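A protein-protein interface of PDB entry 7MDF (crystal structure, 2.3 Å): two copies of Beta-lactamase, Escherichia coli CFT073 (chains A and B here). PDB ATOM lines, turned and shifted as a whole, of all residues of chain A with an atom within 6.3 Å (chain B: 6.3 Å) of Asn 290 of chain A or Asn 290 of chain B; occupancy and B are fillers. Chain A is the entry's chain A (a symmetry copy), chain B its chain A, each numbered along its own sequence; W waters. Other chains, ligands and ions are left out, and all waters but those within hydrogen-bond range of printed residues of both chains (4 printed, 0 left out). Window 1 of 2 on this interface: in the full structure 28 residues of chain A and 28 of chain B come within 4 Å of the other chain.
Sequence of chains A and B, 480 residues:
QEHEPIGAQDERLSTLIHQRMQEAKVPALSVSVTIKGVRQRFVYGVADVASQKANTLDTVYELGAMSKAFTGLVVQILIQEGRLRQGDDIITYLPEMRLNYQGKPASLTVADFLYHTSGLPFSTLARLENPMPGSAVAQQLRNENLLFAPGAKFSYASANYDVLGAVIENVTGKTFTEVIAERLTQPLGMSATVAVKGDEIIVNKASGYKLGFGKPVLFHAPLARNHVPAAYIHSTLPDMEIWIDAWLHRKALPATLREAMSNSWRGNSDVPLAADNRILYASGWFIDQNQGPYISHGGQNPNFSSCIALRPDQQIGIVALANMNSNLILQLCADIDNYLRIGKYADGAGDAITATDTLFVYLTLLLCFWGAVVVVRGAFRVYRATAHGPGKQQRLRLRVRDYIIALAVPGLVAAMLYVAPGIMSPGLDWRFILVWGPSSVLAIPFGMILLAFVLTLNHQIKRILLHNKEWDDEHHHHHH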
ATOM      1  N   LEU A 273      31.208 -24.474 -16.779  1.00  0.00           N
ATOM      2  CA  LEU A 273      30.073 -23.706 -17.262  1.00  0.00           C
ATOM      3  C   LEU A 273      28.825 -24.562 -17.144  1.00  0.00           C
ATOM      4  O   LEU A 273      28.875 -25.773 -17.372  1.00  0.00           O
ATOM      5  CB  LEU A 273      30.281 -23.268 -18.714  1.00  0.00           C
ATOM      6  CG  LEU A 273      31.573 -22.466 -18.937  1.00  0.00           C
ATOM      7  CD1 LEU A 273      31.871 -22.228 -20.424  1.00  0.00           C
ATOM      8  CD2 LEU A 273      31.539 -21.144 -18.173  1.00  0.00           C
ATOM      9  N   ASN A 277      24.363 -21.447 -19.137  1.00  0.00           N
ATOM     10  CA  ASN A 277      25.153 -20.248 -18.895  1.00  0.00           C
ATOM     11  C   ASN A 277      26.629 -20.573 -19.154  1.00  0.00           C
ATOM     12  O   ASN A 277      27.314 -21.152 -18.298  1.00  0.00           O
ATOM     13  CB  ASN A 277      24.916 -19.728 -17.489  1.00  0.00           C
ATOM     14  CG  ASN A 277      25.495 -18.331 -17.276  1.00  0.00           C
ATOM     15  OD1 ASN A 277      26.331 -17.865 -18.052  1.00  0.00           O
ATOM     16  ND2 ASN A 277      25.058 -17.671 -16.218  1.00  0.00           N
ATOM     17  N   ARG A 278      27.102 -20.180 -20.333  1.00  0.00           N
ATOM     18  CA  ARG A 278      28.496 -20.323 -20.724  1.00  0.00           C
ATOM     19  C   ARG A 278      29.163 -18.954 -20.850  1.00  0.00           C
ATOM     20  O   ARG A 278      30.179 -18.810 -21.544  1.00  0.00           O
ATOM     21  CB  ARG A 278      28.605 -21.137 -22.026  1.00  0.00           C
ATOM     22  CG  ARG A 278      28.016 -22.543 -21.922  1.00  0.00           C
ATOM     23  CD  ARG A 278      27.878 -23.264 -23.273  1.00  0.00           C
ATOM     24  NE  ARG A 278      29.133 -23.674 -23.901  1.00  0.00           N
ATOM     25  CZ  ARG A 278      29.774 -24.826 -23.677  1.00  0.00           C
ATOM     26  NH1 ARG A 278      29.400 -25.655 -22.712  1.00  0.00           N
ATOM     27  NH2 ARG A 278      30.805 -25.160 -24.456  1.00  0.00           N
ATOM     28  N   ILE A 279      28.591 -17.948 -20.181  1.00  0.00           N
ATOM     29  CA  ILE A 279      29.143 -16.597 -20.161  1.00  0.00           C
ATOM     30  C   ILE A 279      30.390 -16.554 -19.280  1.00  0.00           C
ATOM     31  O   ILE A 279      30.435 -17.168 -18.203  1.00  0.00           O
ATOM     32  CB  ILE A 279      28.083 -15.609 -19.645  1.00  0.00           C
ATOM     33  CG1 ILE A 279      26.866 -15.573 -20.572  1.00  0.00           C
ATOM     34  CG2 ILE A 279      28.677 -14.211 -19.398  1.00  0.00           C
ATOM     35  CD1 ILE A 279      25.730 -14.731 -19.979  1.00  0.00           C
ATOM     36  N   LEU A 280      31.410 -15.826 -19.729  1.00  0.00           N
ATOM     37  CA  LEU A 280      32.648 -15.661 -18.974  1.00  0.00           C
ATOM     38  C   LEU A 280      32.687 -14.321 -18.240  1.00  0.00           C
ATOM     39  O   LEU A 280      32.068 -13.333 -18.653  1.00  0.00           O
ATOM     40  CB  LEU A 280      33.865 -15.765 -19.896  1.00  0.00           C
ATOM     41  CG  LEU A 280      33.945 -17.007 -20.787  1.00  0.00           C
ATOM     42  CD1 LEU A 280      35.296 -17.014 -21.479  1.00  0.00           C
ATOM     43  CD2 LEU A 280      33.672 -18.326 -19.988  1.00  0.00           C
ATOM     44  N   ILE A 287      31.177 -11.263 -20.214  1.00  0.00           N
ATOM     45  CA  ILE A 287      31.454 -11.348 -21.648  1.00  0.00           C
ATOM     46  C   ILE A 287      30.547 -12.429 -22.207  1.00  0.00           C
ATOM     47  O   ILE A 287      30.589 -13.578 -21.747  1.00  0.00           O
ATOM     48  CB  ILE A 287      32.924 -11.697 -21.946  1.00  0.00           C
ATOM     49  CG1 ILE A 287      33.892 -10.902 -21.045  1.00  0.00           C
ATOM     50  CG2 ILE A 287      33.232 -11.520 -23.448  1.00  0.00           C
ATOM     51  CD1 ILE A 287      33.899  -9.409 -21.279  1.00  0.00           C
ATOM     52  N   ASP A 288      29.716 -12.057 -23.179  1.00  0.00           N
ATOM     53  CA  ASP A 288      28.721 -12.944 -23.760  1.00  0.00           C
ATOM     54  C   ASP A 288      28.876 -12.860 -25.264  1.00  0.00           C
ATOM     55  O   ASP A 288      28.757 -11.772 -25.829  1.00  0.00           O
ATOM     56  CB  ASP A 288      27.309 -12.536 -23.334  1.00  0.00           C
ATOM     57  CG  ASP A 288      26.249 -13.576 -23.691  1.00  0.00           C
ATOM     58  OD1 ASP A 288      26.439 -14.367 -24.660  1.00  0.00           O
ATOM     59  OD2 ASP A 288      25.217 -13.591 -22.978  1.00  0.00           O
ATOM     60  N   GLN A 289      29.159 -13.996 -25.911  1.00  0.00           N
ATOM     61  CA  GLN A 289      29.302 -13.981 -27.363  1.00  0.00           C
ATOM     62  C   GLN A 289      27.970 -14.080 -28.085  1.00  0.00           C
ATOM     63  O   GLN A 289      27.926 -13.843 -29.294  1.00  0.00           O
ATOM     64  CB  GLN A 289      30.208 -15.117 -27.830  1.00  0.00           C
ATOM     65  CG  GLN A 289      31.611 -15.025 -27.331  1.00  0.00           C
ATOM     66  CD  GLN A 289      32.310 -13.764 -27.811  1.00  0.00           C
ATOM     67  OE1 GLN A 289      32.246 -13.411 -28.991  1.00  0.00           O
ATOM     68  NE2 GLN A 289      32.985 -13.083 -26.896  1.00  0.00           N
ATOM     69  N   ASN A 290      26.901 -14.454 -27.385  1.00  0.00           N
ATOM     70  CA  ASN A 290      25.588 -14.589 -28.012  1.00  0.00           C
ATOM     71  C   ASN A 290      25.009 -13.214 -28.382  1.00  0.00           C
ATOM     72  O   ASN A 290      24.932 -12.300 -27.541  1.00  0.00           O
ATOM     73  CB  ASN A 290      24.638 -15.317 -27.068  1.00  0.00           C
ATOM     74  CG  ASN A 290      24.946 -16.782 -26.946  1.00  0.00           C
ATOM     75  OD1 ASN A 290      25.213 -17.461 -27.944  1.00  0.00           O
ATOM     76  ND2 ASN A 290      24.889 -17.296 -25.711  1.00  0.00           N
ATOM     77  N   GLN A 291      24.579 -13.076 -29.640  1.00  0.00           N
ATOM     78  CA  GLN A 291      24.165 -11.773 -30.200  1.00  0.00           C
ATOM     79  C   GLN A 291      25.143 -10.684 -29.775  1.00  0.00           C
ATOM     80  O   GLN A 291      24.747  -9.581 -29.355  1.00  0.00           O
ATOM     81  CB  GLN A 291      22.734 -11.398 -29.787  1.00  0.00           C
ATOM     82  CG  GLN A 291      21.659 -12.374 -30.241  1.00  0.00           C
ATOM     83  CD  GLN A 291      21.773 -12.705 -31.698  1.00  0.00           C
ATOM     84  OE1 GLN A 291      22.089 -13.831 -32.058  1.00  0.00           O
ATOM     85  NE2 GLN A 291      21.541 -11.715 -32.551  1.00  0.00           N
ATOM     86  N   GLY A 292      26.437 -11.023 -29.859  1.00  0.00           N
ATOM     87  CA  GLY A 292      27.481 -10.222 -29.266  1.00  0.00           C
ATOM     88  C   GLY A 292      28.720 -10.033 -30.121  1.00  0.00           C
ATOM     89  O   GLY A 292      28.685 -10.185 -31.345  1.00  0.00           O
ATOM     90  N   PRO A 293      29.865  -9.714 -29.489  1.00  0.00           N
ATOM     91  CA  PRO A 293      30.143  -9.587 -28.054  1.00  0.00           C
ATOM     92  C   PRO A 293      29.216  -8.612 -27.334  1.00  0.00           C
ATOM     93  O   PRO A 293      28.971  -7.508 -27.830  1.00  0.00           O
ATOM     94  CB  PRO A 293      31.587  -9.074 -28.023  1.00  0.00           C
ATOM     95  CG  PRO A 293      32.179  -9.576 -29.291  1.00  0.00           C
ATOM     96  CD  PRO A 293      31.071  -9.472 -30.299  1.00  0.00           C
ATOM     97  N   TYR A 294      28.665  -9.062 -26.209  1.00  0.00           N
ATOM     98  CA  TYR A 294      27.807  -8.255 -25.355  1.00  0.00           C
ATOM     99  C   TYR A 294      28.460  -8.238 -23.980  1.00  0.00           C
ATOM    100  O   TYR A 294      28.469  -9.254 -23.263  1.00  0.00           O
ATOM    101  CB  TYR A 294      26.379  -8.805 -25.313  1.00  0.00           C
ATOM    102  CG  TYR A 294      25.395  -8.019 -24.457  1.00  0.00           C
ATOM    103  CD1 TYR A 294      24.806  -6.852 -24.920  1.00  0.00           C
ATOM    104  CD2 TYR A 294      25.034  -8.470 -23.196  1.00  0.00           C
ATOM    105  CE1 TYR A 294      23.888  -6.144 -24.143  1.00  0.00           C
ATOM    106  CE2 TYR A 294      24.133  -7.768 -22.406  1.00  0.00           C
ATOM    107  CZ  TYR A 294      23.557  -6.608 -22.890  1.00  0.00           C
ATOM    108  OH  TYR A 294      22.645  -5.924 -22.113  1.00  0.00           O
ATOM    109  N   LEU B 273      15.921 -11.065 -25.292  1.00  0.00           N
ATOM    110  CA  LEU B 273      16.888 -11.870 -24.564  1.00  0.00           C
ATOM    111  C   LEU B 273      17.117 -11.237 -23.203  1.00  0.00           C
ATOM    112  O   LEU B 273      17.140 -10.010 -23.082  1.00  0.00           O
ATOM    113  CB  LEU B 273      18.209 -11.973 -25.331  1.00  0.00           C
ATOM    114  CG  LEU B 273      18.053 -12.527 -26.756  1.00  0.00           C
ATOM    115  CD1 LEU B 273      19.345 -12.416 -27.577  1.00  0.00           C
ATOM    116  CD2 LEU B 273      17.546 -13.967 -26.735  1.00  0.00           C
ATOM    117  N   ASN B 277      21.015 -14.475 -20.392  1.00  0.00           N
ATOM    118  CA  ASN B 277      20.670 -15.577 -21.280  1.00  0.00           C
ATOM    119  C   ASN B 277      20.324 -15.005 -22.660  1.00  0.00           C
ATOM    120  O   ASN B 277      19.205 -14.521 -22.887  1.00  0.00           O
ATOM    121  CB  ASN B 277      19.535 -16.398 -20.695  1.00  0.00           C
ATOM    122  CG  ASN B 277      19.321 -17.714 -21.438  1.00  0.00           C
ATOM    123  OD1 ASN B 277      19.794 -17.894 -22.561  1.00  0.00           O
ATOM    124  ND2 ASN B 277      18.599 -18.629 -20.814  1.00  0.00           N
ATOM    125  N   ARG B 278      21.290 -15.082 -23.570  1.00  0.00           N
ATOM    126  CA  ARG B 278      21.120 -14.671 -24.955  1.00  0.00           C
ATOM    127  C   ARG B 278      21.182 -15.881 -25.886  1.00  0.00           C
ATOM    128  O   ARG B 278      21.470 -15.739 -27.083  1.00  0.00           O
ATOM    129  CB  ARG B 278      22.166 -13.605 -25.328  1.00  0.00           C
ATOM    130  CG  ARG B 278      22.090 -12.345 -24.468  1.00  0.00           C
ATOM    131  CD  ARG B 278      23.283 -11.392 -24.649  1.00  0.00           C
ATOM    132  NE  ARG B 278      23.345 -10.694 -25.931  1.00  0.00           N
ATOM    133  CZ  ARG B 278      22.745  -9.533 -26.214  1.00  0.00           C
ATOM    134  NH1 ARG B 278      21.879  -8.976 -25.380  1.00  0.00           N
ATOM    135  NH2 ARG B 278      23.038  -8.910 -27.357  1.00  0.00           N
ATOM    136  N   ILE B 279      20.915 -17.071 -25.338  1.00  0.00           N
ATOM    137  CA  ILE B 279      20.883 -18.308 -26.113  1.00  0.00           C
ATOM    138  C   ILE B 279      19.621 -18.354 -26.973  1.00  0.00           C
ATOM    139  O   ILE B 279      18.529 -17.970 -26.530  1.00  0.00           O
ATOM    140  CB  ILE B 279      20.933 -19.517 -25.163  1.00  0.00           C
ATOM    141  CG1 ILE B 279      22.235 -19.534 -24.361  1.00  0.00           C
ATOM    142  CG2 ILE B 279      20.682 -20.839 -25.908  1.00  0.00           C
ATOM    143  CD1 ILE B 279      22.223 -20.628 -23.286  1.00  0.00           C
ATOM    144  N   LEU B 280      19.763 -18.828 -28.209  1.00  0.00           N
ATOM    145  CA  LEU B 280      18.638 -18.968 -29.129  1.00  0.00           C
ATOM    146  C   LEU B 280      18.134 -20.410 -29.188  1.00  0.00           C
ATOM    147  O   LEU B 280      18.878 -21.370 -28.956  1.00  0.00           O
ATOM    148  CB  LEU B 280      19.028 -18.513 -30.537  1.00  0.00           C
ATOM    149  CG  LEU B 280      19.646 -17.117 -30.659  1.00  0.00           C
ATOM    150  CD1 LEU B 280      19.788 -16.784 -32.133  1.00  0.00           C
ATOM    151  CD2 LEU B 280      18.827 -16.038 -29.874  1.00  0.00           C
ATOM    152  N   ILE B 287      20.928 -23.187 -29.077  1.00  0.00           N
ATOM    153  CA  ILE B 287      22.135 -22.777 -29.795  1.00  0.00           C
ATOM    154  C   ILE B 287      22.831 -21.743 -28.930  1.00  0.00           C
ATOM    155  O   ILE B 287      22.233 -20.715 -28.583  1.00  0.00           O
ATOM    156  CB  ILE B 287      21.823 -22.175 -31.178  1.00  0.00           C
ATOM    157  CG1 ILE B 287      20.750 -22.992 -31.926  1.00  0.00           C
ATOM    158  CG2 ILE B 287      23.117 -22.001 -32.000  1.00  0.00           C
ATOM    159  CD1 ILE B 287      21.171 -24.392 -32.313  1.00  0.00           C
ATOM    160  N   ASP B 288      24.081 -22.022 -28.566  1.00  0.00           N
ATOM    161  CA  ASP B 288      24.857 -21.184 -27.667  1.00  0.00           C
ATOM    162  C   ASP B 288      26.195 -20.941 -28.330  1.00  0.00           C
ATOM    163  O   ASP B 288      26.910 -21.898 -28.629  1.00  0.00           O
ATOM    164  CB  ASP B 288      25.038 -21.861 -26.306  1.00  0.00           C
ATOM    165  CG  ASP B 288      25.609 -20.928 -25.241  1.00  0.00           C
ATOM    166  OD1 ASP B 288      26.322 -19.939 -25.582  1.00  0.00           O
ATOM    167  OD2 ASP B 288      25.328 -21.200 -24.049  1.00  0.00           O
ATOM    168  N   GLN B 289      26.529 -19.669 -28.579  1.00  0.00           N
ATOM    169  CA  GLN B 289      27.815 -19.372 -29.200  1.00  0.00           C
ATOM    170  C   GLN B 289      28.954 -19.315 -28.197  1.00  0.00           C
ATOM    171  O   GLN B 289      30.116 -19.308 -28.609  1.00  0.00           O
ATOM    172  CB  GLN B 289      27.757 -18.050 -29.962  1.00  0.00           C
ATOM    173  CG  GLN B 289      26.797 -18.045 -31.104  1.00  0.00           C
ATOM    174  CD  GLN B 289      27.158 -19.074 -32.163  1.00  0.00           C
ATOM    175  OE1 GLN B 289      28.317 -19.187 -32.571  1.00  0.00           O
ATOM    176  NE2 GLN B 289      26.164 -19.825 -32.615  1.00  0.00           N
ATOM    177  N   ASN B 290      28.648 -19.242 -26.903  1.00  0.00           N
ATOM    178  CA  ASN B 290      29.687 -19.167 -25.878  1.00  0.00           C
ATOM    179  C   ASN B 290      30.430 -20.506 -25.746  1.00  0.00           C
ATOM    180  O   ASN B 290      29.811 -21.572 -25.577  1.00  0.00           O
ATOM    181  CB  ASN B 290      29.065 -18.783 -24.540  1.00  0.00           C
ATOM    182  CG  ASN B 290      28.636 -17.345 -24.488  1.00  0.00           C
ATOM    183  OD1 ASN B 290      29.363 -16.448 -24.931  1.00  0.00           O
ATOM    184  ND2 ASN B 290      27.449 -17.103 -23.918  1.00  0.00           N
ATOM    185  N   GLN B 291      31.765 -20.446 -25.800  1.00  0.00           N
ATOM    186  CA  GLN B 291      32.612 -21.654 -25.869  1.00  0.00           C
ATOM    187  C   GLN B 291      32.014 -22.660 -26.846  1.00  0.00           C
ATOM    188  O   GLN B 291      31.926 -23.869 -26.563  1.00  0.00           O
ATOM    189  CB  GLN B 291      32.807 -22.299 -24.490  1.00  0.00           C
ATOM    190  CG  GLN B 291      33.483 -21.411 -23.455  1.00  0.00           C
ATOM    191  CD  GLN B 291      34.736 -20.781 -23.983  1.00  0.00           C
ATOM    192  OE1 GLN B 291      34.796 -19.573 -24.167  1.00  0.00           O
ATOM    193  NE2 GLN B 291      35.743 -21.601 -24.254  1.00  0.00           N
ATOM    194  N   GLY B 292      31.571 -22.135 -27.997  1.00  0.00           N
ATOM    195  CA  GLY B 292      30.755 -22.886 -28.920  1.00  0.00           C
ATOM    196  C   GLY B 292      31.115 -22.725 -30.385  1.00  0.00           C
ATOM    197  O   GLY B 292      32.233 -22.336 -30.732  1.00  0.00           O
ATOM    198  N   PRO B 293      30.159 -23.002 -31.292  1.00  0.00           N
ATOM    199  CA  PRO B 293      28.754 -23.376 -31.092  1.00  0.00           C
ATOM    200  C   PRO B 293      28.566 -24.596 -30.194  1.00  0.00           C
ATOM    201  O   PRO B 293      29.266 -25.600 -30.357  1.00  0.00           O
ATOM    202  CB  PRO B 293      28.269 -23.679 -32.513  1.00  0.00           C
ATOM    203  CG  PRO B 293      29.150 -22.855 -33.382  1.00  0.00           C
ATOM    204  CD  PRO B 293      30.497 -22.907 -32.721  1.00  0.00           C
ATOM    205  N   TYR B 294      27.670 -24.462 -29.218  1.00  0.00           N
ATOM    206  CA  TYR B 294      27.310 -25.535 -28.304  1.00  0.00           C
ATOM    207  C   TYR B 294      25.808 -25.739 -28.448  1.00  0.00           C
ATOM    208  O   TYR B 294      25.004 -24.896 -28.011  1.00  0.00           O
ATOM    209  CB  TYR B 294      27.716 -25.209 -26.866  1.00  0.00           C
ATOM    210  CG  TYR B 294      27.398 -26.280 -25.831  1.00  0.00           C
ATOM    211  CD1 TYR B 294      28.201 -27.400 -25.680  1.00  0.00           C
ATOM    212  CD2 TYR B 294      26.307 -26.147 -24.985  1.00  0.00           C
ATOM    213  CE1 TYR B 294      27.920 -28.371 -24.717  1.00  0.00           C
ATOM    214  CE2 TYR B 294      26.007 -27.112 -24.033  1.00  0.00           C
ATOM    215  CZ  TYR B 294      26.824 -28.219 -23.899  1.00  0.00           C
ATOM    216  OH  TYR B 294      26.538 -29.165 -22.937  1.00  0.00           O
HETATM  217  O   HOH W   1      32.375 -18.209 -23.405  1.00  0.00           O
HETATM  218  O   HOH W   2      25.723 -18.909 -22.651  1.00  0.00           O
HETATM  219  O   HOH W   3      24.104 -16.040 -23.334  1.00  0.00           O
HETATM  220  O   HOH W   4      22.462 -15.642 -29.850  1.00  0.00           O
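NH2 of Arg 278 of chain A lies within hydrogen-bond range of O of Gln 291 of chain B, at 2.7 Å.
The side-chain amide oxygen (OD1) of Asn 290 of chain B sits at hydrogen-bond distance from the backbone NH (N) of Gln 289 of chain A.
The guanidinium group (NE) of Arg 278 of chain A lies within hydrogen-bond range of the backbone carbonyl oxygen (O) of Asn 290 of chain B.
The side-chain amide nitrogen (ND2) of Asn 290 of chain A lies within hydrogen-bond range of the side-chain carboxylate (OD1) of Asp 288 of chain B (3.0 Å).
The side-chain amide nitrogen (ND2) of Asn 290 of chain B lies within hydrogen-bond range of the side-chain carboxylate (OD1) of Asp 288 of chain A.
The side-chain amide nitrogen of Asn 290 of chain B lies close to the side-chain amide nitrogen of Asn 290 of chain A (3.1 Å).
The side-chain amide oxygen (OD1) of Asn 290 of chain A sits at hydrogen-bond distance from the backbone NH (N) of Gln 289 of chain B (2.6 Å).
The guanidinium group (NE) of Arg 278 of chain B sits at hydrogen-bond distance from the backbone carbonyl oxygen (O) of Asn 290 of chain A.
The guanidinium group (NH2) of Arg 278 of chain B lies within hydrogen-bond range of the backbone carbonyl oxygen (O) of Gln 291 of chain A, at 2.7 Å.
N of Tyr 294 of chain B lies within hydrogen-bond range of O of Asp 288 of chain B (2.7 Å).
The backbone NH (N) of Ile 287 of chain B sits at hydrogen-bond distance from the backbone carbonyl oxygen (O) of Leu 280 of chain B (2.7 Å).
The side-chain amide oxygen of Asn 277 of chain A lies within hydrogen-bond range of the backbone NH of Ile 279 of chain A, 3.1 Å away.
N of Ile 287 of chain A is in hydrogen-bond range of O of Leu 280 of chain A (2.7 Å).
The backbone carbonyl oxygen of Asp 288 of chain A sits at hydrogen-bond distance from the backbone NH of Tyr 294 of chain A, 2.7 Å away.
OD1 of Asn 277 of chain B is in hydrogen-bond range of N of Ile 279 of chain B, 3.1 Å away.
Among the printed residues, merely in contact across the chains: Arg 278 of chain A with Asp 288 of chain B, Asp 288 of chain A with Arg 278 of chain B, Arg 278 of chain A with Tyr 294 of chain B, Tyr 294 of chain A with Arg 278 of chain B, Leu 273 of chain A with Gln 291 of chain B, Gln 291 of chain A with Leu 273 of chain B, Asn 290 of chain A with Ile 279 of chain B, Ile 279 of chain A with Asn 290 of chain B, Gln 291 of chain A with Leu 280 of chain B and Leu 280 of chain A with Gln 291 of chain B.
Asn 290 of chain A touches just these residues of chain B: Arg 278 (2.8 Å), Ile 279 (3.7 Å), Asp 288 (3.0 Å), Gln 289 (2.6 Å) and Asn 290 (3.1 Å).
Printed residues of chain A within 4 Å of Leu 273 of chain B: Gln 291 (3.5 Å).
Of the printed residues of chain B, Leu 280 of chain A touches Gln 291 (3.7 Å).
Of the printed residues of chain B, Leu 273 of chain A touches Gln 291.
Of the printed residues of chain A, Arg 278 of chain B touches Asp 288 (3.4 Å), Asn 290 (2.8 Å), Gln 291 (2.7 Å) and Tyr 294 (3.5 Å).
Of the printed residues of chain B, Gln 289 of chain A touches Asn 290 (2.6 Å).
The nearest residue of chain B that does not touch Asn 290 of chain A is Ile 287 of chain B (4.5 Å).
Of the 13 printed residues of chain A, 9 touch a printed residue of chain B.
Hydrophobic or aromatic side chains of chain A within 4 Å of the printed part of chain B: Leu 273, Ile 279, Leu 280 and Tyr 294.
Printed residues of chain B that touch a printed residue of chain A: Leu 273, Arg 278, Ile 279, Leu 280, Asp 288, Gln 289, Asn 290, Gln 291 and Tyr 294.
Among the printed residues, 19 pairs touch across the chains.
Among the printed residues, no Asp or Glu carboxylate lies within 4 Å of a Lys or Arg side-chain nitrogen of the other chain.
Arg 278 of chain A touches Gln 291 of chain B, and with the chains exchanged Gln 291 of chain A touches Arg 278 of chain B.
Leu 280 of chain A touches Gln 291 of chain B, and with the chains exchanged Gln 291 of chain A touches Leu 280 of chain B.
Gln 289 of chain A touches Asn 290 of chain B, and with the chains exchanged Asn 290 of chain A touches Gln 289 of chain B.
Asn 290 of chain B touches its own counterpart, Asn 290 of chain A.
Water W2 lies within hydrogen-bond range of OD2 of Asp 288 of chain B (2.7 Å), ND2 of Asn 290 of chain B (2.8 Å) and N of Arg 278 of chain A (3.0 Å).
Water W3 lies within hydrogen-bond range of OD2 of Asp 288 of chain A (2.7 Å), ND2 of Asn 290 of chain A (2.8 Å) and N of Arg 278 of chain B (3.0 Å).
Water W1 lies within hydrogen-bond range of OE1 of Gln 291 of chain B (2.9 Å) and O of Arg 278 of chain A (2.9 Å).
Water W4 bridges the side-chain amide oxygen of Gln 291 of chain A and the backbone carbonyl oxygen of Arg 278 of chain B.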
